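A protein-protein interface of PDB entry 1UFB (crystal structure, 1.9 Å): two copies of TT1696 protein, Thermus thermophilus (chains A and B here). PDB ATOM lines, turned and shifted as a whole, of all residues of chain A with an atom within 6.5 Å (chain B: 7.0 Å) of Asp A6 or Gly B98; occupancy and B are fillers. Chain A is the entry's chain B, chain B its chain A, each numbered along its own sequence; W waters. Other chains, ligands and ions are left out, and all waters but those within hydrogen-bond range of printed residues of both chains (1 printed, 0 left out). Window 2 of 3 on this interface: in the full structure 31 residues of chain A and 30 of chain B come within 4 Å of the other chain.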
ATOM      1  N   ASN A   2     -17.822  -5.287 -29.763  1.00  0.00           N
ATOM      2  CA  ASN A   2     -17.301  -5.698 -28.457  1.00  0.00           C
ATOM      3  C   ASN A   2     -18.449  -6.140 -27.506  1.00  0.00           C
ATOM      4  O   ASN A   2     -18.287  -6.148 -26.280  1.00  0.00           O
ATOM      5  CB  ASN A   2     -16.509  -4.551 -27.795  1.00  0.00           C
ATOM      6  CG  ASN A   2     -15.136  -4.300 -28.435  1.00  0.00           C
ATOM      7  OD1 ASN A   2     -14.397  -5.225 -28.751  1.00  0.00           O
ATOM      8  ND2 ASN A   2     -14.778  -3.022 -28.580  1.00  0.00           N
ATOM      9  N   ARG A   3     -19.586  -6.503 -28.097  1.00  0.00           N
ATOM     10  CA  ARG A   3     -20.798  -6.929 -27.395  1.00  0.00           C
ATOM     11  C   ARG A   3     -21.508  -5.795 -26.676  1.00  0.00           C
ATOM     12  O   ARG A   3     -22.431  -6.044 -25.871  1.00  0.00           O
ATOM     13  CB  ARG A   3     -20.495  -8.055 -26.399  1.00  0.00           C
ATOM     14  CG  ARG A   3     -19.982  -9.284 -27.074  1.00  0.00           C
ATOM     15  CD  ARG A   3     -19.970 -10.453 -26.143  1.00  0.00           C
ATOM     16  NE  ARG A   3     -21.327 -10.956 -25.922  1.00  0.00           N
ATOM     17  CZ  ARG A   3     -21.578 -12.014 -25.158  1.00  0.00           C
ATOM     18  NH1 ARG A   3     -20.541 -12.626 -24.585  1.00  0.00           N
ATOM     19  NH2 ARG A   3     -22.837 -12.448 -24.966  1.00  0.00           N
ATOM     20  N   ALA A   4     -21.094  -4.565 -26.968  1.00  0.00           N
ATOM     21  CA  ALA A   4     -21.720  -3.412 -26.342  1.00  0.00           C
ATOM     22  C   ALA A   4     -23.230  -3.589 -26.466  1.00  0.00           C
ATOM     23  O   ALA A   4     -23.998  -3.340 -25.486  1.00  0.00           O
ATOM     24  CB  ALA A   4     -21.291  -2.093 -27.049  1.00  0.00           C
ATOM     25  N   ARG A   5     -23.658  -4.058 -27.646  1.00  0.00           N
ATOM     26  CA  ARG A   5     -25.071  -4.204 -27.908  1.00  0.00           C
ATOM     27  C   ARG A   5     -25.742  -5.274 -27.088  1.00  0.00           C
ATOM     28  O   ARG A   5     -26.931  -5.126 -26.767  1.00  0.00           O
ATOM     29  CB  ARG A   5     -25.347  -4.402 -29.415  1.00  0.00           C
ATOM     30  CG  ARG A   5     -24.988  -3.149 -30.277  1.00  0.00           C
ATOM     31  CD  ARG A   5     -25.850  -1.880 -29.905  1.00  0.00           C
ATOM     32  NE  ARG A   5     -25.646  -0.709 -30.802  1.00  0.00           N
ATOM     33  CZ  ARG A   5     -26.266   0.483 -30.687  1.00  0.00           C
ATOM     34  NH1 ARG A   5     -27.159   0.704 -29.706  1.00  0.00           N
ATOM     35  NH2 ARG A   5     -25.979   1.475 -31.545  1.00  0.00           N
ATOM     36  N   ASP A   6     -25.017  -6.339 -26.751  1.00  0.00           N
ATOM     37  CA  ASP A   6     -25.608  -7.391 -25.920  1.00  0.00           C
ATOM     38  C   ASP A   6     -25.905  -6.806 -24.524  1.00  0.00           C
ATOM     39  O   ASP A   6     -26.970  -7.068 -23.927  1.00  0.00           O
ATOM     40  CB  ASP A   6     -24.679  -8.578 -25.777  1.00  0.00           C
ATOM     41  CG  ASP A   6     -24.509  -9.365 -27.080  1.00  0.00           C
ATOM     42  OD1 ASP A   6     -25.475  -9.472 -27.872  1.00  0.00           O
ATOM     43  OD2 ASP A   6     -23.399  -9.896 -27.276  1.00  0.00           O
ATOM     44  N   TRP A   7     -24.966  -6.021 -24.028  1.00  0.00           N
ATOM     45  CA  TRP A   7     -25.109  -5.351 -22.740  1.00  0.00           C
ATOM     46  C   TRP A   7     -26.233  -4.308 -22.730  1.00  0.00           C
ATOM     47  O   TRP A   7     -26.977  -4.171 -21.724  1.00  0.00           O
ATOM     48  CB  TRP A   7     -23.806  -4.722 -22.355  1.00  0.00           C
ATOM     49  CG  TRP A   7     -22.841  -5.723 -21.942  1.00  0.00           C
ATOM     50  CD1 TRP A   7     -22.063  -6.500 -22.757  1.00  0.00           C
ATOM     51  CD2 TRP A   7     -22.535  -6.123 -20.573  1.00  0.00           C
ATOM     52  NE1 TRP A   7     -21.292  -7.348 -22.001  1.00  0.00           N
ATOM     53  CE2 TRP A   7     -21.554  -7.148 -20.657  1.00  0.00           C
ATOM     54  CE3 TRP A   7     -22.990  -5.712 -19.315  1.00  0.00           C
ATOM     55  CZ2 TRP A   7     -20.997  -7.778 -19.507  1.00  0.00           C
ATOM     56  CZ3 TRP A   7     -22.426  -6.332 -18.145  1.00  0.00           C
ATOM     57  CH2 TRP A   7     -21.435  -7.360 -18.264  1.00  0.00           C
ATOM     58  N   LEU A   8     -26.402  -3.587 -23.848  1.00  0.00           N
ATOM     59  CA  LEU A   8     -27.494  -2.622 -23.921  1.00  0.00           C
ATOM     60  C   LEU A   8     -28.814  -3.375 -23.912  1.00  0.00           C
ATOM     61  O   LEU A   8     -29.747  -2.972 -23.214  1.00  0.00           O
ATOM     62  CB  LEU A   8     -27.360  -1.721 -25.186  1.00  0.00           C
ATOM     63  CG  LEU A   8     -26.755  -0.338 -24.872  1.00  0.00           C
ATOM     64  CD1 LEU A   8     -27.645   0.351 -23.833  1.00  0.00           C
ATOM     65  CD2 LEU A   8     -25.347  -0.434 -24.339  1.00  0.00           C
ATOM     66  N   GLU A   9     -28.908  -4.493 -24.643  1.00  0.00           N
ATOM     67  CA  GLU A   9     -30.144  -5.268 -24.642  1.00  0.00           C
ATOM     68  C   GLU A   9     -30.399  -5.884 -23.258  1.00  0.00           C
ATOM     69  O   GLU A   9     -31.556  -6.015 -22.819  1.00  0.00           O
ATOM     70  CB  GLU A   9     -30.111  -6.372 -25.735  1.00  0.00           C
ATOM     71  CG  GLU A   9     -31.376  -7.315 -25.738  1.00  0.00           C
ATOM     72  CD  GLU A   9     -32.736  -6.613 -25.993  1.00  0.00           C
ATOM     73  OE1 GLU A   9     -32.841  -5.791 -26.940  1.00  0.00           O
ATOM     74  OE2 GLU A   9     -33.708  -6.899 -25.234  1.00  0.00           O
ATOM     75  N   GLN A  10     -29.341  -6.299 -22.574  1.00  0.00           N
ATOM     76  CA  GLN A  10     -29.515  -6.818 -21.193  1.00  0.00           C
ATOM     77  C   GLN A  10     -30.071  -5.625 -20.332  1.00  0.00           C
ATOM     78  O   GLN A  10     -31.054  -5.779 -19.569  1.00  0.00           O
ATOM     79  CB  GLN A  10     -28.179  -7.295 -20.641  1.00  0.00           C
ATOM     80  CG  GLN A  10     -28.297  -7.802 -19.221  1.00  0.00           C
ATOM     81  CD  GLN A  10     -29.211  -9.025 -19.118  1.00  0.00           C
ATOM     82  OE1 GLN A  10     -29.126  -9.934 -19.957  1.00  0.00           O
ATOM     83  NE2 GLN A  10     -30.086  -9.063 -18.093  1.00  0.00           N
ATOM     84  N   ALA A  11     -29.489  -4.442 -20.524  1.00  0.00           N
ATOM     85  CA  ALA A  11     -29.967  -3.239 -19.790  1.00  0.00           C
ATOM     86  C   ALA A  11     -31.435  -2.975 -19.965  1.00  0.00           C
ATOM     87  O   ALA A  11     -32.168  -2.664 -18.962  1.00  0.00           O
ATOM     88  CB  ALA A  11     -29.189  -1.977 -20.184  1.00  0.00           C
ATOM     89  N   TYR B  91     -25.513 -11.397 -16.518  1.00  0.00           N
ATOM     90  CA  TYR B  91     -24.332 -10.825 -17.184  1.00  0.00           C
ATOM     91  C   TYR B  91     -24.063 -11.491 -18.511  1.00  0.00           C
ATOM     92  O   TYR B  91     -23.775 -12.679 -18.554  1.00  0.00           O
ATOM     93  CB  TYR B  91     -23.096 -10.912 -16.259  1.00  0.00           C
ATOM     94  CG  TYR B  91     -23.226  -9.952 -15.089  1.00  0.00           C
ATOM     95  CD1 TYR B  91     -23.460 -10.420 -13.771  1.00  0.00           C
ATOM     96  CD2 TYR B  91     -23.198  -8.566 -15.298  1.00  0.00           C
ATOM     97  CE1 TYR B  91     -23.667  -9.494 -12.662  1.00  0.00           C
ATOM     98  CE2 TYR B  91     -23.407  -7.624 -14.202  1.00  0.00           C
ATOM     99  CZ  TYR B  91     -23.637  -8.126 -12.884  1.00  0.00           C
ATOM    100  OH  TYR B  91     -23.772  -7.249 -11.808  1.00  0.00           O
ATOM    101  N   PRO B  92     -24.115 -10.698 -19.607  1.00  0.00           N
ATOM    102  CA  PRO B  92     -23.903 -11.229 -20.970  1.00  0.00           C
ATOM    103  C   PRO B  92     -22.614 -12.008 -21.184  1.00  0.00           C
ATOM    104  O   PRO B  92     -22.630 -13.061 -21.823  1.00  0.00           O
ATOM    105  CB  PRO B  92     -24.021  -9.988 -21.855  1.00  0.00           C
ATOM    106  CG  PRO B  92     -25.004  -9.121 -21.048  1.00  0.00           C
ATOM    107  CD  PRO B  92     -24.407  -9.240 -19.640  1.00  0.00           C
ATOM    108  N   ASP B  93     -21.518 -11.544 -20.608  1.00  0.00           N
ATOM    109  CA  ASP B  93     -20.241 -12.246 -20.782  1.00  0.00           C
ATOM    110  C   ASP B  93     -20.193 -13.659 -20.144  1.00  0.00           C
ATOM    111  O   ASP B  93     -19.201 -14.345 -20.243  1.00  0.00           O
ATOM    112  CB  ASP B  93     -19.083 -11.375 -20.298  1.00  0.00           C
ATOM    113  CG  ASP B  93     -19.232 -10.925 -18.818  1.00  0.00           C
ATOM    114  OD1 ASP B  93     -20.331 -10.994 -18.187  1.00  0.00           O
ATOM    115  OD2 ASP B  93     -18.231 -10.476 -18.285  1.00  0.00           O
ATOM    116  N   HIS B  95     -22.125 -15.879 -21.273  1.00  0.00           N
ATOM    117  CA  HIS B  95     -22.591 -16.722 -22.393  1.00  0.00           C
ATOM    118  C   HIS B  95     -21.926 -16.320 -23.691  1.00  0.00           C
ATOM    119  O   HIS B  95     -21.470 -15.190 -23.831  1.00  0.00           O
ATOM    120  CB  HIS B  95     -24.081 -16.628 -22.547  1.00  0.00           C
ATOM    121  CG  HIS B  95     -24.815 -16.839 -21.262  1.00  0.00           C
ATOM    122  ND1 HIS B  95     -25.240 -18.077 -20.842  1.00  0.00           N
ATOM    123  CD2 HIS B  95     -25.212 -15.960 -20.311  1.00  0.00           C
ATOM    124  CE1 HIS B  95     -25.880 -17.957 -19.690  1.00  0.00           C
ATOM    125  NE2 HIS B  95     -25.871 -16.682 -19.345  1.00  0.00           N
ATOM    126  N   PRO B  96     -21.840 -17.258 -24.659  1.00  0.00           N
ATOM    127  CA  PRO B  96     -21.191 -16.917 -25.929  1.00  0.00           C
ATOM    128  C   PRO B  96     -21.747 -15.735 -26.646  1.00  0.00           C
ATOM    129  O   PRO B  96     -21.023 -14.930 -27.200  1.00  0.00           O
ATOM    130  CB  PRO B  96     -21.342 -18.197 -26.753  1.00  0.00           C
ATOM    131  CG  PRO B  96     -21.162 -19.285 -25.681  1.00  0.00           C
ATOM    132  CD  PRO B  96     -22.005 -18.717 -24.511  1.00  0.00           C
ATOM    133  N   ALA B  97     -23.048 -15.572 -26.619  1.00  0.00           N
ATOM    134  CA  ALA B  97     -23.565 -14.484 -27.409  1.00  0.00           C
ATOM    135  C   ALA B  97     -24.878 -14.028 -26.861  1.00  0.00           C
ATOM    136  O   ALA B  97     -25.508 -14.751 -26.059  1.00  0.00           O
ATOM    137  CB  ALA B  97     -23.743 -14.984 -28.871  1.00  0.00           C
ATOM    138  N   GLY B  98     -25.287 -12.842 -27.311  1.00  0.00           N
ATOM    139  CA  GLY B  98     -26.544 -12.247 -26.889  1.00  0.00           C
ATOM    140  C   GLY B  98     -26.578 -11.818 -25.413  1.00  0.00           C
ATOM    141  O   GLY B  98     -25.597 -11.971 -24.653  1.00  0.00           O
ATOM    142  N   PRO B  99     -27.704 -11.227 -25.000  1.00  0.00           N
ATOM    143  CA  PRO B  99     -27.854 -10.797 -23.615  1.00  0.00           C
ATOM    144  C   PRO B  99     -28.022 -12.076 -22.768  1.00  0.00           C
ATOM    145  O   PRO B  99     -28.378 -13.148 -23.281  1.00  0.00           O
ATOM    146  CB  PRO B  99     -29.130  -9.974 -23.634  1.00  0.00           C
ATOM    147  CG  PRO B  99     -29.927 -10.623 -24.808  1.00  0.00           C
ATOM    148  CD  PRO B  99     -28.822 -10.764 -25.838  1.00  0.00           C
ATOM    149  N   ALA B 100     -27.779 -11.945 -21.472  1.00  0.00           N
ATOM    150  CA  ALA B 100     -27.923 -13.067 -20.566  1.00  0.00           C
ATOM    151  C   ALA B 100     -29.353 -13.613 -20.554  1.00  0.00           C
ATOM    152  O   ALA B 100     -29.540 -14.813 -20.620  1.00  0.00           O
ATOM    153  CB  ALA B 100     -27.541 -12.621 -19.131  1.00  0.00           C
ATOM    154  N   ALA B 101     -30.339 -12.720 -20.512  1.00  0.00           N
ATOM    155  CA  ALA B 101     -31.771 -13.095 -20.384  1.00  0.00           C
ATOM    156  C   ALA B 101     -32.354 -14.150 -21.309  1.00  0.00           C
ATOM    157  O   ALA B 101     -33.247 -14.952 -20.893  1.00  0.00           O
ATOM    158  CB  ALA B 101     -32.619 -11.830 -20.491  1.00  0.00           C
ATOM    159  N   ARG B 102     -31.838 -14.164 -22.540  1.00  0.00           N
ATOM    160  CA  ARG B 102     -32.352 -15.085 -23.559  1.00  0.00           C
ATOM    161  C   ARG B 102     -31.935 -16.531 -23.377  1.00  0.00           C
ATOM    162  O   ARG B 102     -32.467 -17.419 -24.018  1.00  0.00           O
ATOM    163  CB  ARG B 102     -31.944 -14.629 -24.986  1.00  0.00           C
ATOM    164  CG  ARG B 102     -30.541 -14.914 -25.309  1.00  0.00           C
ATOM    165  CD  ARG B 102     -30.186 -14.654 -26.795  1.00  0.00           C
ATOM    166  NE  ARG B 102     -29.036 -15.504 -27.134  1.00  0.00           N
ATOM    167  CZ  ARG B 102     -28.156 -15.292 -28.112  1.00  0.00           C
ATOM    168  NH1 ARG B 102     -28.259 -14.214 -28.898  1.00  0.00           N
ATOM    169  NH2 ARG B 102     -27.176 -16.184 -28.304  1.00  0.00           N
ATOM    170  N   HIS B 103     -30.974 -16.786 -22.504  1.00  0.00           N
ATOM    171  CA  HIS B 103     -30.539 -18.154 -22.342  1.00  0.00           C
ATOM    172  C   HIS B 103     -31.329 -18.920 -21.302  1.00  0.00           C
ATOM    173  O   HIS B 103     -30.918 -20.024 -20.966  1.00  0.00           O
ATOM    174  CB  HIS B 103     -29.052 -18.183 -21.958  1.00  0.00           C
ATOM    175  CG  HIS B 103     -28.153 -17.624 -23.019  1.00  0.00           C
ATOM    176  ND1 HIS B 103     -27.766 -16.304 -23.052  1.00  0.00           N
ATOM    177  CD2 HIS B 103     -27.595 -18.208 -24.110  1.00  0.00           C
ATOM    178  CE1 HIS B 103     -27.012 -16.092 -24.118  1.00  0.00           C
ATOM    179  NE2 HIS B 103     -26.892 -17.231 -24.776  1.00  0.00           N
HETATM  180  O   HOH W   1     -22.902 -11.498 -29.329  1.00  0.00           O
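No position is printed for both chains.
Of the 10 printed residues of chain A, 5 touch a printed residue of chain B.
Among the printed residues, no Asp or Glu carboxylate lies within 4 Å of a Lys or Arg side-chain nitrogen of the other chain.
The backbone carbonyl oxygen (O) of Ala B97 is in hydrogen-bond range of the guanidinium group (NH2) of Arg B102, 3.1 Å away.
OD2 of Asp A6 is in salt-bridge range of NE of Arg A3, at 2.7 Å.
A ring nitrogen (NE2) of His B103 lies close to the backbone carbonyl oxygen of Ala B97, 3.1 Å away.
ND1 of His B103 lies within hydrogen-bond range of O of Pro B99 (3.2 Å).
O of Ala B100 sits at hydrogen-bond distance from ND1 of His B103.
The side-chain amide oxygen (OE1) of Gln A10 sits at hydrogen-bond distance from the backbone NH (N) of Ala B100, 2.9 Å away.
The side-chain carboxylate of Asp A6 sits close to the backbone NH of Gly B98 (3.4 Å).
O of Gly B98 sits at hydrogen-bond distance from NH2 of Arg A3 (2.8 Å).
OE1 of Gln A10 sits at hydrogen-bond distance from N of Ala B101 (3.1 Å).
The backbone carbonyl oxygen (O) of His B95 lies within hydrogen-bond range of the guanidinium group (NH1) of Arg A3 (2.8 Å).
The backbone carbonyl oxygen (O) of Pro B92 sits at hydrogen-bond distance from the guanidinium group (NH2) of Arg A3 (3.2 Å).
NH1 of Arg A3 touches CA of Asp B93 (3.8 Å).
Pro B96 touches Arg A3 (O to NH1, 3.5 Å).
Ala B97 touches Arg A3.
Pro B99 touches Asp A6 (CB to O, 3.6 Å).
CH2 of Trp A7 touches CD2 of Tyr B91, at 3.7 Å.
Trp A7 touches Pro B92.
Trp A7 touches Asp B93.
CG of Pro B99 touches CG of Glu A9 (3.7 Å).
Pro B92 touches Gln A10 (CG to CB, 3.7 Å).
OE1 of Gln A10 touches CB of Pro B99 (3.7 Å).
Ala A4 touches none of the printed residues of chain B.
Asp A6 touches just these residues of chain B: Gly B98 and Pro B99.
Printed residues of chain B within 4 Å of Gln A10: Pro B92, Pro B99, Ala B100 and Ala B101.
Printed residues of chain A within 4 Å of Pro B92: Arg A3 (3.2 Å), Trp A7 (3.7 Å) and Gln A10 (3.7 Å).
Of the printed residues of chain A, Asp B93 touches Arg A3 and Trp A7.
Of the printed residues of chain A, Pro B96 touches Arg A3 (3.5 Å).
Of chain A, only Arg A3 and Asp A6 come within 4 Å of Gly B98.
Printed residues of chain A within 4 Å of Pro B99: Asp A6, Glu A9 and Gln A10.
His B103 touches none of the printed residues of chain A.
The nearest residue of chain B that does not touch Asp A6 is Pro B92 (4.05 Å).
The nearest residue of chain A that does not touch Gly B98 is Trp A7 (6.0 Å).
The nearest printed residue of chain B that does not touch Glu A9 is Ala B101 (6.4 Å).
Water W1 lies within hydrogen-bond range of the side-chain carboxylate of Asp A6 (2.7 Å) and the backbone NH of Gly B98 (3.4 Å).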
